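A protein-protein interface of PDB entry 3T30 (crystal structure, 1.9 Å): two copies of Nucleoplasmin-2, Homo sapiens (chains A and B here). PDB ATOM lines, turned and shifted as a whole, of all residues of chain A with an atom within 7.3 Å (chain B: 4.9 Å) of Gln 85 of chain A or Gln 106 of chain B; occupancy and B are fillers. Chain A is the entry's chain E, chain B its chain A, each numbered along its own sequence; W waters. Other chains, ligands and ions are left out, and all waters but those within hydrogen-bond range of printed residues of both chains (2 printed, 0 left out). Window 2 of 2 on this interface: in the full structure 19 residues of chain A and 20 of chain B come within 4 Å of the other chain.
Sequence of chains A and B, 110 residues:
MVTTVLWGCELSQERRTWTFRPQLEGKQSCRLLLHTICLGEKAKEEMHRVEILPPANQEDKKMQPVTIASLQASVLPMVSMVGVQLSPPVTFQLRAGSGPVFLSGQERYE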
ATOM      1  N   CYS A  30      30.978  -6.958 -26.766  1.00  0.00           N
ATOM      2  CA  CYS A  30      31.206  -7.181 -25.353  1.00  0.00           C
ATOM      3  C   CYS A  30      29.886  -6.994 -24.605  1.00  0.00           C
ATOM      4  O   CYS A  30      29.861  -6.849 -23.379  1.00  0.00           O
ATOM      5  CB  CYS A  30      32.263  -6.204 -24.841  1.00  0.00           C
ATOM      6  SG  CYS A  30      32.246  -4.610 -25.708  1.00  0.00           S
ATOM      7  N   ARG A  31      28.792  -6.982 -25.363  1.00  0.00           N
ATOM      8  CA  ARG A  31      27.453  -7.030 -24.795  1.00  0.00           C
ATOM      9  C   ARG A  31      26.487  -7.749 -25.742  1.00  0.00           C
ATOM     10  O   ARG A  31      26.376  -7.407 -26.916  1.00  0.00           O
ATOM     11  CB  ARG A  31      26.928  -5.625 -24.491  1.00  0.00           C
ATOM     12  CG  ARG A  31      27.544  -4.977 -23.268  1.00  0.00           C
ATOM     13  CD  ARG A  31      27.190  -5.723 -21.991  1.00  0.00           C
ATOM     14  NE  ARG A  31      27.530  -4.922 -20.814  1.00  0.00           N
ATOM     15  CZ  ARG A  31      26.932  -5.019 -19.625  1.00  0.00           C
ATOM     16  NH1 ARG A  31      25.945  -5.892 -19.420  1.00  0.00           N
ATOM     17  NH2 ARG A  31      27.333  -4.236 -18.630  1.00  0.00           N
ATOM     18  N   LEU A  32      25.823  -8.761 -25.205  1.00  0.00           N
ATOM     19  CA  LEU A  32      24.771  -9.459 -25.900  1.00  0.00           C
ATOM     20  C   LEU A  32      23.420  -8.860 -25.439  1.00  0.00           C
ATOM     21  O   LEU A  32      23.023  -9.036 -24.283  1.00  0.00           O
ATOM     22  CB  LEU A  32      24.793 -10.924 -25.501  1.00  0.00           C
ATOM     23  CG  LEU A  32      24.105 -11.846 -26.508  1.00  0.00           C
ATOM     24  CD1 LEU A  32      25.107 -12.080 -27.639  1.00  0.00           C
ATOM     25  CD2 LEU A  32      23.725 -13.180 -25.876  1.00  0.00           C
ATOM     26  N   LEU A  33      22.733  -8.166 -26.336  1.00  0.00           N
ATOM     27  CA  LEU A  33      21.378  -7.693 -26.036  1.00  0.00           C
ATOM     28  C   LEU A  33      20.452  -8.860 -26.336  1.00  0.00           C
ATOM     29  O   LEU A  33      20.430  -9.333 -27.496  1.00  0.00           O
ATOM     30  CB  LEU A  33      21.026  -6.504 -26.933  1.00  0.00           C
ATOM     31  CG  LEU A  33      21.510  -5.089 -26.583  1.00  0.00           C
ATOM     32  CD1 LEU A  33      22.718  -5.042 -25.656  1.00  0.00           C
ATOM     33  CD2 LEU A  33      21.760  -4.276 -27.848  1.00  0.00           C
ATOM     34  N   LEU A  34      19.735  -9.361 -25.328  1.00  0.00           N
ATOM     35  CA  LEU A  34      18.796 -10.467 -25.546  1.00  0.00           C
ATOM     36  C   LEU A  34      17.409  -9.929 -25.829  1.00  0.00           C
ATOM     37  O   LEU A  34      16.837  -9.261 -24.971  1.00  0.00           O
ATOM     38  CB  LEU A  34      18.762 -11.397 -24.340  1.00  0.00           C
ATOM     39  CG  LEU A  34      17.832 -12.607 -24.370  1.00  0.00           C
ATOM     40  CD1 LEU A  34      18.256 -13.577 -25.557  1.00  0.00           C
ATOM     41  CD2 LEU A  34      17.867 -13.359 -23.033  1.00  0.00           C
ATOM     42  N   MET A  81      12.080  -9.859 -24.044  1.00  0.00           N
ATOM     43  CA  MET A  81      12.719  -9.244 -22.880  1.00  0.00           C
ATOM     44  C   MET A  81      13.701  -8.184 -23.330  1.00  0.00           C
ATOM     45  O   MET A  81      14.840  -8.123 -22.831  1.00  0.00           O
ATOM     46  CB  MET A  81      13.457 -10.288 -22.036  1.00  0.00           C
ATOM     47  CG  MET A  81      14.374 -11.191 -22.819  1.00  0.00           C
ATOM     48  SD  MET A  81      14.804 -12.540 -21.676  1.00  0.00           S
ATOM     49  CE  MET A  81      13.270 -13.461 -21.703  1.00  0.00           C
ATOM     50  N   VAL A  82      13.260  -7.371 -24.283  1.00  0.00           N
ATOM     51  CA  VAL A  82      14.108  -6.334 -24.834  1.00  0.00           C
ATOM     52  C   VAL A  82      14.584  -5.482 -23.646  1.00  0.00           C
ATOM     53  O   VAL A  82      13.791  -5.022 -22.833  1.00  0.00           O
ATOM     54  CB  VAL A  82      13.344  -5.531 -25.926  1.00  0.00           C
ATOM     55  CG1 VAL A  82      14.166  -4.361 -26.506  1.00  0.00           C
ATOM     56  CG2 VAL A  82      12.910  -6.487 -27.041  1.00  0.00           C
ATOM     57  N   GLY A  83      15.882  -5.274 -23.577  1.00  0.00           N
ATOM     58  CA  GLY A  83      16.478  -4.502 -22.507  1.00  0.00           C
ATOM     59  C   GLY A  83      17.516  -5.295 -21.722  1.00  0.00           C
ATOM     60  O   GLY A  83      18.368  -4.714 -21.054  1.00  0.00           O
ATOM     61  N   VAL A  84      17.437  -6.622 -21.772  1.00  0.00           N
ATOM     62  CA  VAL A  84      18.440  -7.442 -21.081  1.00  0.00           C
ATOM     63  C   VAL A  84      19.760  -7.404 -21.823  1.00  0.00           C
ATOM     64  O   VAL A  84      19.787  -7.631 -23.021  1.00  0.00           O
ATOM     65  CB  VAL A  84      18.029  -8.892 -21.031  1.00  0.00           C
ATOM     66  CG1 VAL A  84      19.198  -9.722 -20.473  1.00  0.00           C
ATOM     67  CG2 VAL A  84      16.779  -9.023 -20.161  1.00  0.00           C
ATOM     68  N   GLN A  85      20.846  -7.113 -21.105  1.00  0.00           N
ATOM     69  CA  GLN A  85      22.177  -7.018 -21.695  1.00  0.00           C
ATOM     70  C   GLN A  85      23.078  -7.953 -20.914  1.00  0.00           C
ATOM     71  O   GLN A  85      23.153  -7.836 -19.708  1.00  0.00           O
ATOM     72  CB  GLN A  85      22.745  -5.620 -21.559  1.00  0.00           C
ATOM     73  CG  GLN A  85      21.892  -4.537 -22.145  1.00  0.00           C
ATOM     74  CD  GLN A  85      22.740  -3.352 -22.588  1.00  0.00           C
ATOM     75  OE1 GLN A  85      22.215  -2.296 -22.958  1.00  0.00           O
ATOM     76  NE2 GLN A  85      24.070  -3.526 -22.552  1.00  0.00           N
ATOM     77  N   LEU A  86      23.762  -8.863 -21.595  1.00  0.00           N
ATOM     78  CA  LEU A  86      24.511  -9.900 -20.918  1.00  0.00           C
ATOM     79  C   LEU A  86      26.001  -9.776 -21.250  1.00  0.00           C
ATOM     80  O   LEU A  86      26.385  -9.353 -22.343  1.00  0.00           O
ATOM     81  CB  LEU A  86      23.989 -11.289 -21.323  1.00  0.00           C
ATOM     82  CG  LEU A  86      22.483 -11.575 -21.134  1.00  0.00           C
ATOM     83  CD1 LEU A  86      22.030 -12.790 -21.872  1.00  0.00           C
ATOM     84  CD2 LEU A  86      22.122 -11.731 -19.660  1.00  0.00           C
ATOM     85  N   SER A  87      26.851 -10.161 -20.310  1.00  0.00           N
ATOM     86  CA  SER A  87      28.289 -10.087 -20.550  1.00  0.00           C
ATOM     87  C   SER A  87      28.793 -11.443 -20.992  1.00  0.00           C
ATOM     88  O   SER A  87      28.600 -12.427 -20.294  1.00  0.00           O
ATOM     89  CB  SER A  87      29.019  -9.642 -19.267  1.00  0.00           C
ATOM     90  OG  SER A  87      28.433  -8.456 -18.743  1.00  0.00           O
ATOM     91  N   VAL A  90      28.319 -16.158 -22.791  1.00  0.00           N
ATOM     92  CA  VAL A  90      27.017 -16.517 -22.247  1.00  0.00           C
ATOM     93  C   VAL A  90      26.715 -17.888 -22.788  1.00  0.00           C
ATOM     94  O   VAL A  90      26.757 -18.067 -23.987  1.00  0.00           O
ATOM     95  CB  VAL A  90      25.897 -15.551 -22.733  1.00  0.00           C
ATOM     96  CG1 VAL A  90      24.580 -15.886 -22.040  1.00  0.00           C
ATOM     97  CG2 VAL A  90      26.299 -14.113 -22.516  1.00  0.00           C
ATOM     98  N   ARG A 108      26.497  -6.183 -29.465  1.00  0.00           N
ATOM     99  CA  ARG A 108      26.701  -4.752 -29.309  1.00  0.00           C
ATOM    100  C   ARG A 108      28.156  -4.469 -28.952  1.00  0.00           C
ATOM    101  O   ARG A 108      28.785  -3.624 -29.595  1.00  0.00           O
ATOM    102  CB  ARG A 108      25.772  -4.171 -28.227  1.00  0.00           C
ATOM    103  CG  ARG A 108      25.964  -2.661 -27.994  1.00  0.00           C
ATOM    104  CD  ARG A 108      25.005  -2.098 -26.940  1.00  0.00           C
ATOM    105  NE  ARG A 108      25.536  -2.205 -25.575  1.00  0.00           N
ATOM    106  CZ  ARG A 108      25.693  -1.175 -24.739  1.00  0.00           C
ATOM    107  NH1 ARG A 108      25.350   0.056 -25.118  1.00  0.00           N
ATOM    108  NH2 ARG A 108      26.188  -1.378 -23.519  1.00  0.00           N
ATOM    109  N   THR B   4      25.895  -6.136 -13.940  1.00  0.00           N
ATOM    110  CA  THR B   4      27.275  -6.591 -14.054  1.00  0.00           C
ATOM    111  C   THR B   4      27.391  -8.082 -13.753  1.00  0.00           C
ATOM    112  O   THR B   4      28.110  -8.809 -14.438  1.00  0.00           O
ATOM    113  CB  THR B   4      28.207  -5.813 -13.106  1.00  0.00           C
ATOM    114  OG1 THR B   4      27.868  -4.420 -13.136  1.00  0.00           O
ATOM    115  CG2 THR B   4      29.659  -5.986 -13.523  1.00  0.00           C
ATOM    116  N   VAL B   5      26.679  -8.530 -12.724  1.00  0.00           N
ATOM    117  CA  VAL B   5      26.701  -9.933 -12.331  1.00  0.00           C
ATOM    118  C   VAL B   5      25.318 -10.565 -12.459  1.00  0.00           C
ATOM    119  O   VAL B   5      24.332 -10.030 -11.952  1.00  0.00           O
ATOM    120  CB  VAL B   5      27.201 -10.106 -10.885  1.00  0.00           C
ATOM    121  CG1 VAL B   5      26.309  -9.342  -9.920  1.00  0.00           C
ATOM    122  CG2 VAL B   5      27.257 -11.581 -10.516  1.00  0.00           C
ATOM    123  N   LEU B   6      25.255 -11.704 -13.139  1.00  0.00           N
ATOM    124  CA  LEU B   6      23.997 -12.410 -13.334  1.00  0.00           C
ATOM    125  C   LEU B   6      23.494 -12.937 -11.992  1.00  0.00           C
ATOM    126  O   LEU B   6      24.273 -13.392 -11.170  1.00  0.00           O
ATOM    127  CB  LEU B   6      24.170 -13.534 -14.374  1.00  0.00           C
ATOM    128  CG  LEU B   6      22.912 -14.198 -14.904  1.00  0.00           C
ATOM    129  CD1 LEU B   6      22.013 -13.171 -15.578  1.00  0.00           C
ATOM    130  CD2 LEU B   6      23.306 -15.290 -15.918  1.00  0.00           C
ATOM    131  N   TRP B   7      22.184 -12.866 -11.787  1.00  0.00           N
ATOM    132  CA  TRP B   7      21.577 -13.329 -10.545  1.00  0.00           C
ATOM    133  C   TRP B   7      20.355 -14.201 -10.817  1.00  0.00           C
ATOM    134  O   TRP B   7      19.695 -14.059 -11.846  1.00  0.00           O
ATOM    135  CB  TRP B   7      21.189 -12.142  -9.662  1.00  0.00           C
ATOM    136  CG  TRP B   7      20.349 -12.522  -8.482  1.00  0.00           C
ATOM    137  CD1 TRP B   7      20.789 -12.985  -7.275  1.00  0.00           C
ATOM    138  CD2 TRP B   7      18.920 -12.470  -8.393  1.00  0.00           C
ATOM    139  NE1 TRP B   7      19.724 -13.224  -6.442  1.00  0.00           N
ATOM    140  CE2 TRP B   7      18.565 -12.916  -7.105  1.00  0.00           C
ATOM    141  CE3 TRP B   7      17.907 -12.089  -9.278  1.00  0.00           C
ATOM    142  CZ2 TRP B   7      17.240 -12.993  -6.679  1.00  0.00           C
ATOM    143  CZ3 TRP B   7      16.592 -12.166  -8.853  1.00  0.00           C
ATOM    144  CH2 TRP B   7      16.270 -12.614  -7.567  1.00  0.00           C
ATOM    145  N   ARG B  31      22.050  -2.338  -6.745  1.00  0.00           N
ATOM    146  CA  ARG B  31      20.828  -2.385  -7.532  1.00  0.00           C
ATOM    147  C   ARG B  31      20.549  -3.783  -8.118  1.00  0.00           C
ATOM    148  O   ARG B  31      21.373  -4.328  -8.824  1.00  0.00           O
ATOM    149  CB  ARG B  31      20.963  -1.386  -8.678  1.00  0.00           C
ATOM    150  CG  ARG B  31      19.659  -0.893  -9.189  1.00  0.00           C
ATOM    151  CD  ARG B  31      18.810  -0.533  -7.993  1.00  0.00           C
ATOM    152  NE  ARG B  31      19.437   0.515  -7.203  1.00  0.00           N
ATOM    153  CZ  ARG B  31      19.053   1.785  -7.260  1.00  0.00           C
ATOM    154  NH1 ARG B  31      18.049   2.125  -8.078  1.00  0.00           N
ATOM    155  NH2 ARG B  31      19.662   2.703  -6.508  1.00  0.00           N
ATOM    156  N   LEU B  32      19.390  -4.347  -7.809  1.00  0.00           N
ATOM    157  CA  LEU B  32      18.950  -5.598  -8.401  1.00  0.00           C
ATOM    158  C   LEU B  32      18.116  -5.248  -9.651  1.00  0.00           C
ATOM    159  O   LEU B  32      17.046  -4.657  -9.520  1.00  0.00           O
ATOM    160  CB  LEU B  32      18.081  -6.381  -7.404  1.00  0.00           C
ATOM    161  CG  LEU B  32      17.749  -7.862  -7.654  1.00  0.00           C
ATOM    162  CD1 LEU B  32      16.582  -7.996  -8.608  1.00  0.00           C
ATOM    163  CD2 LEU B  32      18.965  -8.614  -8.200  1.00  0.00           C
ATOM    164  N   LEU B  33      18.620  -5.563 -10.845  1.00  0.00           N
ATOM    165  CA  LEU B  33      17.781  -5.444 -12.051  1.00  0.00           C
ATOM    166  C   LEU B  33      17.029  -6.738 -12.226  1.00  0.00           C
ATOM    167  O   LEU B  33      17.629  -7.769 -12.477  1.00  0.00           O
ATOM    168  CB  LEU B  33      18.601  -5.174 -13.290  1.00  0.00           C
ATOM    169  CG  LEU B  33      19.777  -4.205 -13.247  1.00  0.00           C
ATOM    170  CD1 LEU B  33      20.121  -3.763 -14.655  1.00  0.00           C
ATOM    171  CD2 LEU B  33      19.504  -3.011 -12.369  1.00  0.00           C
ATOM    172  N   HIS B  35      14.675  -9.248 -14.138  1.00  0.00           N
ATOM    173  CA  HIS B  35      14.341  -9.484 -15.555  1.00  0.00           C
ATOM    174  C   HIS B  35      13.098 -10.312 -15.869  1.00  0.00           C
ATOM    175  O   HIS B  35      12.174  -9.816 -16.514  1.00  0.00           O
ATOM    176  CB  HIS B  35      15.559 -10.019 -16.281  1.00  0.00           C
ATOM    177  CG  HIS B  35      16.624  -8.982 -16.419  1.00  0.00           C
ATOM    178  ND1 HIS B  35      17.962  -9.284 -16.547  1.00  0.00           N
ATOM    179  CD2 HIS B  35      16.531  -7.631 -16.453  1.00  0.00           C
ATOM    180  CE1 HIS B  35      18.646  -8.163 -16.685  1.00  0.00           C
ATOM    181  NE2 HIS B  35      17.802  -7.145 -16.612  1.00  0.00           N
ATOM    182  N   SER B 104      15.111 -14.202 -12.344  1.00  0.00           N
ATOM    183  CA  SER B 104      16.371 -13.867 -12.941  1.00  0.00           C
ATOM    184  C   SER B 104      16.573 -12.377 -12.929  1.00  0.00           C
ATOM    185  O   SER B 104      15.604 -11.596 -12.874  1.00  0.00           O
ATOM    186  CB  SER B 104      16.447 -14.350 -14.414  1.00  0.00           C
ATOM    187  OG  SER B 104      15.524 -13.601 -15.229  1.00  0.00           O
ATOM    188  N   GLY B 105      17.835 -11.967 -13.007  1.00  0.00           N
ATOM    189  CA  GLY B 105      18.139 -10.547 -13.120  1.00  0.00           C
ATOM    190  C   GLY B 105      19.626 -10.337 -13.012  1.00  0.00           C
ATOM    191  O   GLY B 105      20.389 -11.279 -13.201  1.00  0.00           O
ATOM    192  N   GLN B 106      20.042  -9.101 -12.768  1.00  0.00           N
ATOM    193  CA  GLN B 106      21.456  -8.800 -12.668  1.00  0.00           C
ATOM    194  C   GLN B 106      21.691  -7.885 -11.476  1.00  0.00           C
ATOM    195  O   GLN B 106      20.893  -6.991 -11.209  1.00  0.00           O
ATOM    196  CB  GLN B 106      22.001  -8.140 -13.941  1.00  0.00           C
ATOM    197  CG  GLN B 106      21.994  -9.073 -15.124  1.00  0.00           C
ATOM    198  CD  GLN B 106      22.182  -8.345 -16.432  1.00  0.00           C
ATOM    199  OE1 GLN B 106      21.449  -7.407 -16.755  1.00  0.00           O
ATOM    200  NE2 GLN B 106      23.162  -8.786 -17.201  1.00  0.00           N
ATOM    201  N   GLU B 107      22.775  -8.156 -10.755  1.00  0.00           N
ATOM    202  CA  GLU B 107      23.260  -7.267  -9.707  1.00  0.00           C
ATOM    203  C   GLU B 107      24.121  -6.226 -10.401  1.00  0.00           C
ATOM    204  O   GLU B 107      25.010  -6.582 -11.161  1.00  0.00           O
ATOM    205  CB  GLU B 107      24.131  -8.042  -8.737  1.00  0.00           C
ATOM    206  CG  GLU B 107      23.495  -9.271  -8.160  1.00  0.00           C
ATOM    207  CD  GLU B 107      24.482 -10.050  -7.284  1.00  0.00           C
ATOM    208  OE1 GLU B 107      25.615  -9.530  -7.077  1.00  0.00           O
ATOM    209  OE2 GLU B 107      24.124 -11.158  -6.800  1.00  0.00           O
ATOM    210  N   ARG B 108      23.888  -4.943 -10.147  1.00  0.00           N
ATOM    211  CA  ARG B 108      24.617  -3.924 -10.909  1.00  0.00           C
ATOM    212  C   ARG B 108      25.580  -3.103 -10.056  1.00  0.00           C
ATOM    213  O   ARG B 108      25.175  -2.540  -9.046  1.00  0.00           O
ATOM    214  CB  ARG B 108      23.651  -3.009 -11.665  1.00  0.00           C
ATOM    215  CG  ARG B 108      24.324  -2.279 -12.803  1.00  0.00           C
ATOM    216  CD  ARG B 108      23.447  -1.166 -13.340  1.00  0.00           C
ATOM    217  NE  ARG B 108      24.239  -0.154 -14.043  1.00  0.00           N
ATOM    218  CZ  ARG B 108      23.856   1.111 -14.209  1.00  0.00           C
ATOM    219  NH1 ARG B 108      22.679   1.518 -13.725  1.00  0.00           N
ATOM    220  NH2 ARG B 108      24.651   1.967 -14.857  1.00  0.00           N
HETATM  221  O   HOH W   1      20.776  -5.741 -18.442  1.00  0.00           O
HETATM  222  O   HOH W   2      25.569 -10.674 -17.386  1.00  0.00           O
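Positions printed for both chains: 31, 32, 33 and 108.
O of Gln 85 of chain A sits at hydrogen-bond distance from NH1 of Arg 31 of chain A, 3.4 Å away. The backbone carbonyl oxygen (O) of Leu 32 of chain A sits at hydrogen-bond distance from the backbone NH (N) of Leu 86 of chain A (2.8 Å). The backbone NH of Leu 34 of chain A sits at hydrogen-bond distance from the backbone carbonyl oxygen of Val 84 of chain A (2.9 Å). The side-chain amide nitrogen of Gln 85 of chain A lies close to the guanidinium group of Arg 108 of chain A. O of Gln 106 of chain B is in hydrogen-bond range of N of Leu 33 of chain B. The backbone carbonyl oxygen (O) of Ser 104 of chain B sits at hydrogen-bond distance from the backbone NH (N) of His 35 of chain B (2.8 Å).
The backbone carbonyl oxygen (O) of Gln 85 of chain A lies within hydrogen-bond range of the side-chain amide nitrogen (NE2) of Gln 106 of chain B (2.7 Å).
Cys 30 of chain A touches none of the printed residues of chain B. Of chain B, only Gln 106 comes within 4 Å of Gln 85 of chain A. Of the printed residues of chain B, Leu 86 of chain A touches Gln 106 (3.98 Å). Printed residues of chain A within 4 Å of His 35 of chain B: Val 84 (3.7 Å). Gln 106 of chain B touches two residues of chain A. The nearest printed residue of chain B that does not touch Leu 86 of chain A is Leu 6 of chain B (4.3 Å).
Hydrophobic or aromatic side chains of chain B that line the printed part of chain A: His 35. Of the 14 printed residues of chain A, 3 touch a printed residue of chain B. Among the printed residues, 3 pairs touch across the chains. Among the printed residues, no Asp or Glu carboxylate lies within 4 Å of a Lys or Arg side-chain nitrogen of the other chain.
Water W1 lies within hydrogen-bond range of OE1 of Gln 106 of chain B (2.5 Å) and N of Gln 85 of chain A (3.0 Å). Water W2 bridges NE2 of Gln 106 of chain B (3.1 Å) and N of Ser 87 of chain A (3.2 Å).
Among the printed residues, merely in contact across the chains: Val 84 of chain A with His 35 of chain B (3.7 Å) and Leu 86 of chain A with Gln 106 of chain B (3.98 Å).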
